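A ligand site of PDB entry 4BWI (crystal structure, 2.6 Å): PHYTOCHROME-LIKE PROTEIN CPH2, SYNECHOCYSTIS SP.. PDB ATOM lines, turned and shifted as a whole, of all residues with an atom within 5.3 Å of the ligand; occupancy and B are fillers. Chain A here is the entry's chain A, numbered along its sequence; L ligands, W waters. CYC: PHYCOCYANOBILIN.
The side-chain hydroxyl of Thr 144 sits at hydrogen-bond distance from an oxygen (O2A) of the ligand (3.5 Å). A nitrogen (ND) of the ligand is in hydrogen-bond range of the backbone carbonyl oxygen (O) of Asp 79 (3.2 Å). SG of Cys 129 is covalently linked to CAC of the ligand, at 1.8 Å. NE2 of His 130 sits at hydrogen-bond distance from O1A of the ligand, at 3.1 Å. NE2 of His 160 lies close to OB of the ligand (3.2 Å). The side-chain amino group (NZ) of Lys 104 is in salt-bridge range of an oxygen (O2D) of the ligand (3.1 Å).
NH2 of Arg 373 lies within salt-bridge range of OD1 of Asp 79 (3.0 Å). The backbone NH (N) of Cys 129 sits at hydrogen-bond distance from the side-chain carboxylate (OD1) of Asp 127, 2.8 Å away. The side-chain carboxylate of Asp 79 is in hydrogen-bond range of the side-chain hydroxyl of Tyr 133. A ring nitrogen (NE2) of His 160 lies within hydrogen-bond range of the side-chain hydroxyl (OG) of Ser 142 (3.3 Å). The backbone NH (N) of Val 97 sits at hydrogen-bond distance from the backbone carbonyl oxygen (O) of Ser 142 (2.6 Å). The backbone carbonyl oxygen of Tyr 47 lies within hydrogen-bond range of the backbone NH of Ile 156 (2.9 Å). The backbone carbonyl oxygen (O) of Phe 75 is in hydrogen-bond range of the side-chain hydroxyl (OH) of Tyr 47 (3.1 Å). A ring nitrogen (ND1) of His 160 is in hydrogen-bond range of the side-chain amino group (NZ) of Lys 45, 3.4 Å away.
Merely in contact with the ligand: Tyr 133 (3.2 Å), Pro 81 (3.2 Å), Ile 380 (3.4 Å), Val 97 (3.4 Å), Gln 83 (3.4 Å), Asn 379 (3.5 Å), Ile 80 (3.5 Å), Val 126 (3.5 Å), Phe 75 (3.6 Å), Asp 127 (3.6 Å), Ala 158 (3.6 Å), Tyr 47 (3.6 Å), Glu 78 (3.7 Å), Ile 95 (3.7 Å), Ile 156 (3.7 Å), Ala 84 (3.7 Å), Arg 373 (3.9 Å) and Lys 45 (3.9 Å). Hydrophobic or aromatic side chains within 4 Å of the ligand: Tyr 47, Phe 75, Ile 80, Pro 81, Ala 84, Ile 95, Val 97, Val 126, His 130, Tyr 133, Ile 156, Ala 158 and His 160. Of the 33 residues printed, 24 come within 4 Å of the ligand. The nearest printed residue that does not touch the ligand is Leu 381 (4.1 Å).
Water W3 lies within hydrogen-bond range of O2A of the ligand (2.5 Å), O of Ile 95 (2.9 Å), OG of Ser 142 (2.9 Å) and OG1 of Thr 144 (3.1 Å). Water W5 lies within hydrogen-bond range of O of Thr 125 (2.6 Å), O1D of the ligand (2.7 Å) and NZ of Lys 104 (3.5 Å). Water W4 lies within hydrogen-bond range of O2A of the ligand, NE2 of His 130 and OG of Ser 142. Water W2 lies within hydrogen-bond range of ND1 of His 130 (2.7 Å), NA of the ligand (2.9 Å) and O of Asp 79 (3.3 Å). Water W1 bridges an oxygen (OC) of the ligand and the guanidinium group of Arg 383.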
ATOM      1  N   LYS A  45     -25.843  -2.574  16.791  1.00  0.00           N
ATOM      2  CA  LYS A  45     -24.696  -2.574  17.691  1.00  0.00           C
ATOM      3  C   LYS A  45     -24.667  -1.358  18.615  1.00  0.00           C
ATOM      4  O   LYS A  45     -25.338  -0.351  18.356  1.00  0.00           O
ATOM      5  CB  LYS A  45     -23.390  -2.617  16.892  1.00  0.00           C
ATOM      6  CG  LYS A  45     -23.217  -3.873  16.049  1.00  0.00           C
ATOM      7  CD  LYS A  45     -22.105  -3.685  15.024  1.00  0.00           C
ATOM      8  CE  LYS A  45     -22.401  -2.500  14.108  1.00  0.00           C
ATOM      9  NZ  LYS A  45     -23.796  -2.534  13.585  1.00  0.00           N
ATOM     10  N   TYR A  47     -21.509   0.912  20.322  1.00  0.00           N
ATOM     11  CA  TYR A  47     -20.074   1.121  20.173  1.00  0.00           C
ATOM     12  C   TYR A  47     -19.649   2.228  21.133  1.00  0.00           C
ATOM     13  O   TYR A  47     -20.250   3.303  21.158  1.00  0.00           O
ATOM     14  CB  TYR A  47     -19.805   1.524  18.722  1.00  0.00           C
ATOM     15  CG  TYR A  47     -18.363   1.782  18.333  1.00  0.00           C
ATOM     16  CD1 TYR A  47     -17.458   0.743  18.192  1.00  0.00           C
ATOM     17  CD2 TYR A  47     -17.914   3.068  18.060  1.00  0.00           C
ATOM     18  CE1 TYR A  47     -16.149   0.974  17.812  1.00  0.00           C
ATOM     19  CE2 TYR A  47     -16.614   3.315  17.681  1.00  0.00           C
ATOM     20  CZ  TYR A  47     -15.726   2.265  17.554  1.00  0.00           C
ATOM     21  OH  TYR A  47     -14.431   2.494  17.184  1.00  0.00           O
ATOM     22  N   VAL A  57     -17.040  -2.598  20.162  1.00  0.00           N
ATOM     23  CA  VAL A  57     -18.428  -3.012  20.100  1.00  0.00           C
ATOM     24  C   VAL A  57     -18.777  -3.741  21.392  1.00  0.00           C
ATOM     25  O   VAL A  57     -18.287  -4.835  21.649  1.00  0.00           O
ATOM     26  CB  VAL A  57     -18.692  -3.916  18.880  1.00  0.00           C
ATOM     27  CG1 VAL A  57     -20.150  -4.347  18.835  1.00  0.00           C
ATOM     28  CG2 VAL A  57     -18.310  -3.187  17.583  1.00  0.00           C
ATOM     29  N   PHE A  75     -12.283  -0.782  16.782  1.00  0.00           N
ATOM     30  CA  PHE A  75     -12.119  -0.007  15.563  1.00  0.00           C
ATOM     31  C   PHE A  75     -11.257   1.214  15.871  1.00  0.00           C
ATOM     32  O   PHE A  75     -11.423   1.832  16.924  1.00  0.00           O
ATOM     33  CB  PHE A  75     -13.467   0.434  14.996  1.00  0.00           C
ATOM     34  CG  PHE A  75     -14.309  -0.690  14.459  1.00  0.00           C
ATOM     35  CD1 PHE A  75     -14.993  -1.534  15.316  1.00  0.00           C
ATOM     36  CD2 PHE A  75     -14.422  -0.900  13.091  1.00  0.00           C
ATOM     37  CE1 PHE A  75     -15.774  -2.572  14.825  1.00  0.00           C
ATOM     38  CE2 PHE A  75     -15.201  -1.929  12.595  1.00  0.00           C
ATOM     39  CZ  PHE A  75     -15.877  -2.769  13.464  1.00  0.00           C
ATOM     40  N   GLU A  78      -9.462   6.646  13.086  1.00  0.00           N
ATOM     41  CA  GLU A  78      -9.573   7.186  11.728  1.00  0.00           C
ATOM     42  C   GLU A  78     -10.854   6.775  11.015  1.00  0.00           C
ATOM     43  O   GLU A  78     -11.245   7.403  10.026  1.00  0.00           O
ATOM     44  CB  GLU A  78      -8.351   6.806  10.883  1.00  0.00           C
ATOM     45  CG  GLU A  78      -7.031   7.321  11.415  1.00  0.00           C
ATOM     46  CD  GLU A  78      -6.437   6.431  12.485  1.00  0.00           C
ATOM     47  OE1 GLU A  78      -6.973   5.319  12.707  1.00  0.00           O
ATOM     48  OE2 GLU A  78      -5.423   6.824  13.101  1.00  0.00           O
ATOM     49  N   ASP A  79     -11.505   5.716  11.499  1.00  0.00           N
ATOM     50  CA  ASP A  79     -12.744   5.242  10.891  1.00  0.00           C
ATOM     51  C   ASP A  79     -13.839   6.316  10.945  1.00  0.00           C
ATOM     52  O   ASP A  79     -14.649   6.431  10.031  1.00  0.00           O
ATOM     53  CB  ASP A  79     -13.229   3.965  11.564  1.00  0.00           C
ATOM     54  CG  ASP A  79     -12.437   2.746  11.124  1.00  0.00           C
ATOM     55  OD1 ASP A  79     -11.285   2.908  10.678  1.00  0.00           O
ATOM     56  OD2 ASP A  79     -12.964   1.626  11.247  1.00  0.00           O
ATOM     57  N   ILE A  80     -13.845   7.088  12.027  1.00  0.00           N
ATOM     58  CA  ILE A  80     -14.778   8.212  12.159  1.00  0.00           C
ATOM     59  C   ILE A  80     -14.013   9.533  12.245  1.00  0.00           C
ATOM     60  O   ILE A  80     -13.486   9.886  13.293  1.00  0.00           O
ATOM     61  CB  ILE A  80     -15.667   8.060  13.404  1.00  0.00           C
ATOM     62  CG1 ILE A  80     -16.218   6.631  13.501  1.00  0.00           C
ATOM     63  CG2 ILE A  80     -16.800   9.070  13.381  1.00  0.00           C
ATOM     64  CD1 ILE A  80     -17.076   6.393  14.709  1.00  0.00           C
ATOM     65  N   PRO A  81     -13.959  10.262  11.122  1.00  0.00           N
ATOM     66  CA  PRO A  81     -13.217  11.532  10.984  1.00  0.00           C
ATOM     67  C   PRO A  81     -13.861  12.665  11.792  1.00  0.00           C
ATOM     68  O   PRO A  81     -15.027  12.540  12.166  1.00  0.00           O
ATOM     69  CB  PRO A  81     -13.306  11.813   9.476  1.00  0.00           C
ATOM     70  CG  PRO A  81     -14.561  11.160   9.052  1.00  0.00           C
ATOM     71  CD  PRO A  81     -14.692   9.921   9.890  1.00  0.00           C
ATOM     72  N   GLN A  83     -15.100  15.496  11.067  1.00  0.00           N
ATOM     73  CA  GLN A  83     -16.339  16.017  10.490  1.00  0.00           C
ATOM     74  C   GLN A  83     -17.559  15.270  11.004  1.00  0.00           C
ATOM     75  O   GLN A  83     -18.577  15.882  11.358  1.00  0.00           O
ATOM     76  CB  GLN A  83     -16.269  15.950   8.963  1.00  0.00           C
ATOM     77  CG  GLN A  83     -15.701  14.643   8.428  1.00  0.00           C
ATOM     78  CD  GLN A  83     -15.735  14.546   6.919  1.00  0.00           C
ATOM     79  OE1 GLN A  83     -16.607  15.117   6.266  1.00  0.00           O
ATOM     80  NE2 GLN A  83     -14.772  13.829   6.354  1.00  0.00           N
ATOM     81  N   ALA A  84     -17.461  13.942  11.060  1.00  0.00           N
ATOM     82  CA  ALA A  84     -18.573  13.096  11.490  1.00  0.00           C
ATOM     83  C   ALA A  84     -18.793  13.171  12.991  1.00  0.00           C
ATOM     84  O   ALA A  84     -19.937  13.248  13.453  1.00  0.00           O
ATOM     85  CB  ALA A  84     -18.328  11.657  11.055  1.00  0.00           C
ATOM     86  N   LEU A  88     -22.133  14.298  14.947  1.00  0.00           N
ATOM     87  CA  LEU A  88     -22.745  13.332  15.858  1.00  0.00           C
ATOM     88  C   LEU A  88     -22.849  13.858  17.285  1.00  0.00           C
ATOM     89  O   LEU A  88     -23.869  13.677  17.950  1.00  0.00           O
ATOM     90  CB  LEU A  88     -21.973  12.007  15.853  1.00  0.00           C
ATOM     91  CG  LEU A  88     -22.051  11.144  14.593  1.00  0.00           C
ATOM     92  CD1 LEU A  88     -21.065   9.994  14.688  1.00  0.00           C
ATOM     93  CD2 LEU A  88     -23.463  10.617  14.390  1.00  0.00           C
ATOM     94  N   ILE A  95     -27.540   9.934  11.875  1.00  0.00           N
ATOM     95  CA  ILE A  95     -27.170   9.903  10.454  1.00  0.00           C
ATOM     96  C   ILE A  95     -27.648   8.629   9.768  1.00  0.00           C
ATOM     97  O   ILE A  95     -27.314   7.524  10.184  1.00  0.00           O
ATOM     98  CB  ILE A  95     -25.644  10.035  10.252  1.00  0.00           C
ATOM     99  CG1 ILE A  95     -25.140  11.319  10.926  1.00  0.00           C
ATOM    100  CG2 ILE A  95     -25.304  10.025   8.764  1.00  0.00           C
ATOM    101  CD1 ILE A  95     -23.657  11.566  10.742  1.00  0.00           C
ATOM    102  N   VAL A  97     -27.542   6.543   6.277  1.00  0.00           N
ATOM    103  CA  VAL A  97     -26.802   6.431   5.023  1.00  0.00           C
ATOM    104  C   VAL A  97     -27.442   5.446   4.061  1.00  0.00           C
ATOM    105  O   VAL A  97     -27.544   4.251   4.348  1.00  0.00           O
ATOM    106  CB  VAL A  97     -25.326   6.024   5.257  1.00  0.00           C
ATOM    107  CG1 VAL A  97     -24.655   5.694   3.925  1.00  0.00           C
ATOM    108  CG2 VAL A  97     -24.567   7.119   5.981  1.00  0.00           C
ATOM    109  N   LYS A 104     -26.918  10.488   2.112  1.00  0.00           N
ATOM    110  CA  LYS A 104     -27.173  10.471   3.552  1.00  0.00           C
ATOM    111  C   LYS A 104     -28.181  11.539   3.937  1.00  0.00           C
ATOM    112  O   LYS A 104     -28.442  12.464   3.170  1.00  0.00           O
ATOM    113  CB  LYS A 104     -25.879  10.723   4.326  1.00  0.00           C
ATOM    114  CG  LYS A 104     -25.272  12.091   4.053  1.00  0.00           C
ATOM    115  CD  LYS A 104     -24.040  12.335   4.888  1.00  0.00           C
ATOM    116  CE  LYS A 104     -23.378  13.661   4.522  1.00  0.00           C
ATOM    117  NZ  LYS A 104     -22.172  13.932   5.348  1.00  0.00           N
ATOM    118  N   THR A 125     -24.750  13.862  -0.634  1.00  0.00           N
ATOM    119  CA  THR A 125     -23.895  12.839  -1.222  1.00  0.00           C
ATOM    120  C   THR A 125     -22.817  12.367  -0.238  1.00  0.00           C
ATOM    121  O   THR A 125     -22.206  13.166   0.461  1.00  0.00           O
ATOM    122  CB  THR A 125     -23.247  13.317  -2.535  1.00  0.00           C
ATOM    123  OG1 THR A 125     -22.358  12.301  -3.024  1.00  0.00           O
ATOM    124  CG2 THR A 125     -22.465  14.611  -2.311  1.00  0.00           C
ATOM    125  N   VAL A 126     -22.602  11.055  -0.176  1.00  0.00           N
ATOM    126  CA  VAL A 126     -21.664  10.461   0.764  1.00  0.00           C
ATOM    127  C   VAL A 126     -20.276  10.298   0.160  1.00  0.00           C
ATOM    128  O   VAL A 126     -20.137   9.934  -1.000  1.00  0.00           O
ATOM    129  CB  VAL A 126     -22.176   9.099   1.280  1.00  0.00           C
ATOM    130  CG1 VAL A 126     -21.144   8.428   2.192  1.00  0.00           C
ATOM    131  CG2 VAL A 126     -23.503   9.269   1.999  1.00  0.00           C
ATOM    132  N   ASP A 127     -19.249  10.598   0.964  1.00  0.00           N
ATOM    133  CA  ASP A 127     -17.856  10.401   0.570  1.00  0.00           C
ATOM    134  C   ASP A 127     -17.623   8.955   0.136  1.00  0.00           C
ATOM    135  O   ASP A 127     -18.156   8.026   0.736  1.00  0.00           O
ATOM    136  CB  ASP A 127     -16.937  10.737   1.741  1.00  0.00           C
ATOM    137  CG  ASP A 127     -15.466  10.742   1.353  1.00  0.00           C
ATOM    138  OD1 ASP A 127     -14.873   9.640   1.272  1.00  0.00           O
ATOM    139  OD2 ASP A 127     -14.902  11.837   1.135  1.00  0.00           O
ATOM    140  N   CYS A 129     -15.139   6.981   0.348  1.00  0.00           N
ATOM    141  CA  CYS A 129     -14.429   6.122   1.296  1.00  0.00           C
ATOM    142  C   CYS A 129     -15.418   5.390   2.197  1.00  0.00           C
ATOM    143  O   CYS A 129     -15.333   4.180   2.382  1.00  0.00           O
ATOM    144  CB  CYS A 129     -13.439   6.929   2.137  1.00  0.00           C
ATOM    145  SG  CYS A 129     -12.592   5.953   3.410  1.00  0.00           S
ATOM    146  N   HIS A 130     -16.363   6.145   2.755  1.00  0.00           N
ATOM    147  CA  HIS A 130     -17.362   5.568   3.657  1.00  0.00           C
ATOM    148  C   HIS A 130     -18.303   4.629   2.905  1.00  0.00           C
ATOM    149  O   HIS A 130     -18.884   3.725   3.503  1.00  0.00           O
ATOM    150  CB  HIS A 130     -18.141   6.673   4.379  1.00  0.00           C
ATOM    151  CG  HIS A 130     -19.014   6.177   5.486  1.00  0.00           C
ATOM    152  ND1 HIS A 130     -18.556   5.346   6.479  1.00  0.00           N
ATOM    153  CD2 HIS A 130     -20.322   6.399   5.754  1.00  0.00           C
ATOM    154  CE1 HIS A 130     -19.537   5.068   7.316  1.00  0.00           C
ATOM    155  NE2 HIS A 130     -20.622   5.697   6.900  1.00  0.00           N
ATOM    156  N   TYR A 133     -16.255   1.462   2.500  1.00  0.00           N
ATOM    157  CA  TYR A 133     -16.194   0.979   3.871  1.00  0.00           C
ATOM    158  C   TYR A 133     -17.452   0.193   4.222  1.00  0.00           C
ATOM    159  O   TYR A 133     -17.378  -0.942   4.679  1.00  0.00           O
ATOM    160  CB  TYR A 133     -16.033   2.186   4.808  1.00  0.00           C
ATOM    161  CG  TYR A 133     -15.886   1.869   6.279  1.00  0.00           C
ATOM    162  CD1 TYR A 133     -17.002   1.714   7.096  1.00  0.00           C
ATOM    163  CD2 TYR A 133     -14.633   1.780   6.865  1.00  0.00           C
ATOM    164  CE1 TYR A 133     -16.873   1.442   8.442  1.00  0.00           C
ATOM    165  CE2 TYR A 133     -14.494   1.507   8.215  1.00  0.00           C
ATOM    166  CZ  TYR A 133     -15.612   1.347   8.998  1.00  0.00           C
ATOM    167  OH  TYR A 133     -15.480   1.083  10.340  1.00  0.00           O
ATOM    168  N   LEU A 134     -18.607   0.813   3.996  1.00  0.00           N
ATOM    169  CA  LEU A 134     -19.879   0.172   4.282  1.00  0.00           C
ATOM    170  C   LEU A 134     -20.138  -1.020   3.362  1.00  0.00           C
ATOM    171  O   LEU A 134     -20.772  -1.988   3.761  1.00  0.00           O
ATOM    172  CB  LEU A 134     -21.028   1.183   4.207  1.00  0.00           C
ATOM    173  CG  LEU A 134     -21.076   2.166   5.380  1.00  0.00           C
ATOM    174  CD1 LEU A 134     -22.208   3.173   5.217  1.00  0.00           C
ATOM    175  CD2 LEU A 134     -21.224   1.414   6.697  1.00  0.00           C
ATOM    176  N   MET A 137     -18.428  -4.040   4.530  1.00  0.00           N
ATOM    177  CA  MET A 137     -19.113  -4.616   5.680  1.00  0.00           C
ATOM    178  C   MET A 137     -20.342  -5.416   5.277  1.00  0.00           C
ATOM    179  O   MET A 137     -20.964  -6.080   6.115  1.00  0.00           O
ATOM    180  CB  MET A 137     -19.530  -3.516   6.665  1.00  0.00           C
ATOM    181  CG  MET A 137     -18.411  -3.034   7.559  1.00  0.00           C
ATOM    182  SD  MET A 137     -19.038  -2.019   8.912  1.00  0.00           S
ATOM    183  CE  MET A 137     -17.536  -1.783   9.861  1.00  0.00           C
ATOM    184  N   SER A 142     -27.575   2.124   6.697  1.00  0.00           N
ATOM    185  CA  SER A 142     -26.962   2.429   7.993  1.00  0.00           C
ATOM    186  C   SER A 142     -27.630   3.609   8.697  1.00  0.00           C
ATOM    187  O   SER A 142     -27.892   4.650   8.086  1.00  0.00           O
ATOM    188  CB  SER A 142     -25.468   2.702   7.820  1.00  0.00           C
ATOM    189  OG  SER A 142     -24.862   2.993   9.064  1.00  0.00           O
ATOM    190  N   THR A 144     -26.795   5.714  12.155  1.00  0.00           N
ATOM    191  CA  THR A 144     -25.913   5.941  13.298  1.00  0.00           C
ATOM    192  C   THR A 144     -26.582   6.869  14.303  1.00  0.00           C
ATOM    193  O   THR A 144     -26.948   8.003  13.968  1.00  0.00           O
ATOM    194  CB  THR A 144     -24.577   6.570  12.868  1.00  0.00           C
ATOM    195  OG1 THR A 144     -23.887   5.673  11.980  1.00  0.00           O
ATOM    196  CG2 THR A 144     -23.710   6.851  14.083  1.00  0.00           C
ATOM    197  N   ILE A 156     -21.810   5.397  19.952  1.00  0.00           N
ATOM    198  CA  ILE A 156     -22.923   5.414  19.015  1.00  0.00           C
ATOM    199  C   ILE A 156     -23.741   4.141  19.125  1.00  0.00           C
ATOM    200  O   ILE A 156     -23.274   3.123  19.627  1.00  0.00           O
ATOM    201  CB  ILE A 156     -22.456   5.545  17.556  1.00  0.00           C
ATOM    202  CG1 ILE A 156     -21.507   4.401  17.191  1.00  0.00           C
ATOM    203  CG2 ILE A 156     -21.796   6.902  17.314  1.00  0.00           C
ATOM    204  CD1 ILE A 156     -21.181   4.307  15.714  1.00  0.00           C
ATOM    205  N   ALA A 158     -25.391   1.661  16.433  1.00  0.00           N
ATOM    206  CA  ALA A 158     -25.281   1.413  15.009  1.00  0.00           C
ATOM    207  C   ALA A 158     -26.331   0.423  14.522  1.00  0.00           C
ATOM    208  O   ALA A 158     -26.400  -0.705  15.002  1.00  0.00           O
ATOM    209  CB  ALA A 158     -23.879   0.923  14.659  1.00  0.00           C
ATOM    210  N   HIS A 160     -27.538  -1.535  11.271  1.00  0.00           N
ATOM    211  CA  HIS A 160     -27.090  -1.932   9.952  1.00  0.00           C
ATOM    212  C   HIS A 160     -27.991  -2.969   9.303  1.00  0.00           C
ATOM    213  O   HIS A 160     -28.509  -3.867   9.971  1.00  0.00           O
ATOM    214  CB  HIS A 160     -25.649  -2.456  10.009  1.00  0.00           C
ATOM    215  CG  HIS A 160     -24.627  -1.398  10.273  1.00  0.00           C
ATOM    216  ND1 HIS A 160     -23.282  -1.673  10.375  1.00  0.00           N
ATOM    217  CD2 HIS A 160     -24.751  -0.063  10.442  1.00  0.00           C
ATOM    218  CE1 HIS A 160     -22.619  -0.551  10.601  1.00  0.00           C
ATOM    219  NE2 HIS A 160     -23.493   0.445  10.656  1.00  0.00           N
ATOM    220  N   ARG A 373      -5.170  -2.734  10.915  1.00  0.00           N
ATOM    221  CA  ARG A 373      -4.941  -1.297  10.940  1.00  0.00           C
ATOM    222  C   ARG A 373      -3.484  -0.987  11.245  1.00  0.00           C
ATOM    223  O   ARG A 373      -2.841  -0.225  10.520  1.00  0.00           O
ATOM    224  CB  ARG A 373      -5.852  -0.624  11.968  1.00  0.00           C
ATOM    225  CG  ARG A 373      -5.372   0.741  12.448  1.00  0.00           C
ATOM    226  CD  ARG A 373      -5.406   1.799  11.347  1.00  0.00           C
ATOM    227  NE  ARG A 373      -6.755   2.071  10.880  1.00  0.00           N
ATOM    228  CZ  ARG A 373      -7.141   3.222  10.342  1.00  0.00           C
ATOM    229  NH1 ARG A 373      -6.271   4.217  10.217  1.00  0.00           N
ATOM    230  NH2 ARG A 373      -8.397   3.383   9.937  1.00  0.00           N
ATOM    231  N   ASN A 379      -5.203   5.658   5.565  1.00  0.00           N
ATOM    232  CA  ASN A 379      -4.749   6.858   4.859  1.00  0.00           C
ATOM    233  C   ASN A 379      -5.787   7.369   3.862  1.00  0.00           C
ATOM    234  O   ASN A 379      -6.812   7.934   4.254  1.00  0.00           O
ATOM    235  CB  ASN A 379      -3.417   6.601   4.156  1.00  0.00           C
ATOM    236  N   ILE A 380      -5.510   7.178   2.572  1.00  0.00           N
ATOM    237  CA  ILE A 380      -6.397   7.662   1.519  1.00  0.00           C
ATOM    238  C   ILE A 380      -7.500   6.656   1.196  1.00  0.00           C
ATOM    239  O   ILE A 380      -8.585   7.044   0.744  1.00  0.00           O
ATOM    240  CB  ILE A 380      -5.610   7.972   0.230  1.00  0.00           C
ATOM    241  N   LEU A 381      -7.227   5.379   1.427  1.00  0.00           N
ATOM    242  CA  LEU A 381      -8.178   4.328   1.105  1.00  0.00           C
ATOM    243  C   LEU A 381      -8.593   3.563   2.357  1.00  0.00           C
ATOM    244  O   LEU A 381      -7.792   3.368   3.268  1.00  0.00           O
ATOM    245  CB  LEU A 381      -7.565   3.354   0.091  1.00  0.00           C
ATOM    246  CG  LEU A 381      -7.069   3.990  -1.207  1.00  0.00           C
ATOM    247  CD1 LEU A 381      -6.578   2.925  -2.173  1.00  0.00           C
ATOM    248  CD2 LEU A 381      -8.164   4.837  -1.836  1.00  0.00           C
ATOM    249  N   PRO A 382      -9.868   3.121   2.395  1.00  0.00           N
ATOM    250  CA  PRO A 382     -10.365   2.328   3.526  1.00  0.00           C
ATOM    251  C   PRO A 382      -9.942   0.865   3.393  1.00  0.00           C
ATOM    252  O   PRO A 382      -9.826   0.357   2.276  1.00  0.00           O
ATOM    253  CB  PRO A 382     -11.876   2.440   3.375  1.00  0.00           C
ATOM    254  CG  PRO A 382     -12.088   2.603   1.908  1.00  0.00           C
ATOM    255  CD  PRO A 382     -10.918   3.408   1.409  1.00  0.00           C
ATOM    256  N   ARG A 383      -9.725   0.197   4.519  1.00  0.00           N
ATOM    257  CA  ARG A 383      -9.457  -1.237   4.488  1.00  0.00           C
ATOM    258  C   ARG A 383     -10.727  -1.965   4.045  1.00  0.00           C
ATOM    259  O   ARG A 383     -11.843  -1.521   4.333  1.00  0.00           O
ATOM    260  CB  ARG A 383      -8.975  -1.744   5.851  1.00  0.00           C
ATOM    261  CG  ARG A 383      -9.973  -1.630   6.986  1.00  0.00           C
ATOM    262  CD  ARG A 383      -9.329  -1.943   8.320  1.00  0.00           C
ATOM    263  NE  ARG A 383     -10.300  -1.951   9.415  1.00  0.00           N
ATOM    264  CZ  ARG A 383     -10.748  -0.854  10.016  1.00  0.00           C
ATOM    265  NH1 ARG A 383     -10.313   0.337   9.642  1.00  0.00           N
ATOM    266  NH2 ARG A 383     -11.633  -0.958  10.997  1.00  0.00           N
HETATM  267  CHA CYC L   1     -18.455   8.402   8.456  1.00  0.00           C
HETATM  268  NA  CYC L   1     -17.712   6.291   9.568  1.00  0.00           N
HETATM  269  C1A CYC L   1     -18.539   7.410   9.526  1.00  0.00           C
HETATM  270  C2A CYC L   1     -19.483   7.551  10.563  1.00  0.00           C
HETATM  271  C3A CYC L   1     -19.291   6.380  11.446  1.00  0.00           C
HETATM  272  C4A CYC L   1     -18.132   5.566  10.782  1.00  0.00           C
HETATM  273  CMA CYC L   1     -20.037   6.072  12.673  1.00  0.00           C
HETATM  274  CAA CYC L   1     -20.481   8.645  10.757  1.00  0.00           C
HETATM  275  CBA CYC L   1     -21.860   8.364  10.418  1.00  0.00           C
HETATM  276  CGA CYC L   1     -22.075   7.806   9.018  1.00  0.00           C
HETATM  277  O1A CYC L   1     -21.526   8.426   7.989  1.00  0.00           O
HETATM  278  O2A CYC L   1     -22.801   6.717   8.841  1.00  0.00           O
HETATM  279  CHB CYC L   1     -17.523   4.274  11.288  1.00  0.00           C
HETATM  280  NB  CYC L   1     -19.598   3.072  11.673  1.00  0.00           N
HETATM  281  C1B CYC L   1     -18.271   3.263  11.899  1.00  0.00           C
HETATM  282  C2B CYC L   1     -17.630   2.301  12.857  1.00  0.00           C
HETATM  283  C3B CYC L   1     -18.857   1.390  13.253  1.00  0.00           C
HETATM  284  C4B CYC L   1     -19.958   2.004  12.440  1.00  0.00           C
HETATM  285  CMB CYC L   1     -16.146   2.223  13.348  1.00  0.00           C
HETATM  286  CAB CYC L   1     -18.883   0.219  14.192  1.00  0.00           C
HETATM  287  CBB CYC L   1     -19.856   0.262  15.315  1.00  0.00           C
HETATM  288  OB  CYC L   1     -21.065   1.583  12.458  1.00  0.00           O
HETATM  289  NC  CYC L   1     -13.559   5.963   6.763  1.00  0.00           N
HETATM  290  C1C CYC L   1     -12.422   5.116   6.810  1.00  0.00           C
HETATM  291  C2C CYC L   1     -11.166   5.657   6.189  1.00  0.00           C
HETATM  292  C3C CYC L   1     -11.667   7.090   5.636  1.00  0.00           C
HETATM  293  C4C CYC L   1     -13.036   7.170   6.245  1.00  0.00           C
HETATM  294  CMC CYC L   1      -9.951   5.629   7.096  1.00  0.00           C
HETATM  295  CAC CYC L   1     -11.605   7.234   4.196  1.00  0.00           C
HETATM  296  CBC CYC L   1     -10.150   7.135   3.711  1.00  0.00           C
HETATM  297  OC  CYC L   1     -12.453   4.028   7.322  1.00  0.00           O
HETATM  298  CHD CYC L   1     -13.701   8.408   6.278  1.00  0.00           C
HETATM  299  ND  CYC L   1     -15.982   8.080   7.580  1.00  0.00           N
HETATM  300  C1D CYC L   1     -15.181   8.698   6.691  1.00  0.00           C
HETATM  301  C2D CYC L   1     -15.879   9.758   6.135  1.00  0.00           C
HETATM  302  C3D CYC L   1     -17.134   9.766   6.718  1.00  0.00           C
HETATM  303  C4D CYC L   1     -17.183   8.707   7.611  1.00  0.00           C
HETATM  304  CMD CYC L   1     -15.368  10.713   5.102  1.00  0.00           C
HETATM  305  CAD CYC L   1     -18.292  10.769   6.398  1.00  0.00           C
HETATM  306  CBD CYC L   1     -19.306  10.328   5.420  1.00  0.00           C
HETATM  307  CGD CYC L   1     -19.936  11.363   4.564  1.00  0.00           C
HETATM  308  O1D CYC L   1     -19.232  12.357   4.119  1.00  0.00           O
HETATM  309  O2D CYC L   1     -21.116  11.271   4.277  1.00  0.00           O
HETATM  310  O   HOH W   1     -10.313   1.966   7.034  1.00  0.00           O
HETATM  311  O   HOH W   2     -16.201   4.772   7.589  1.00  0.00           O
HETATM  312  O   HOH W   3     -25.155   5.924   9.181  1.00  0.00           O
HETATM  313  O   HOH W   4     -21.914   4.115   9.268  1.00  0.00           O
HETATM  314  O   HOH W   5     -20.539  13.896   2.257  1.00  0.00           O
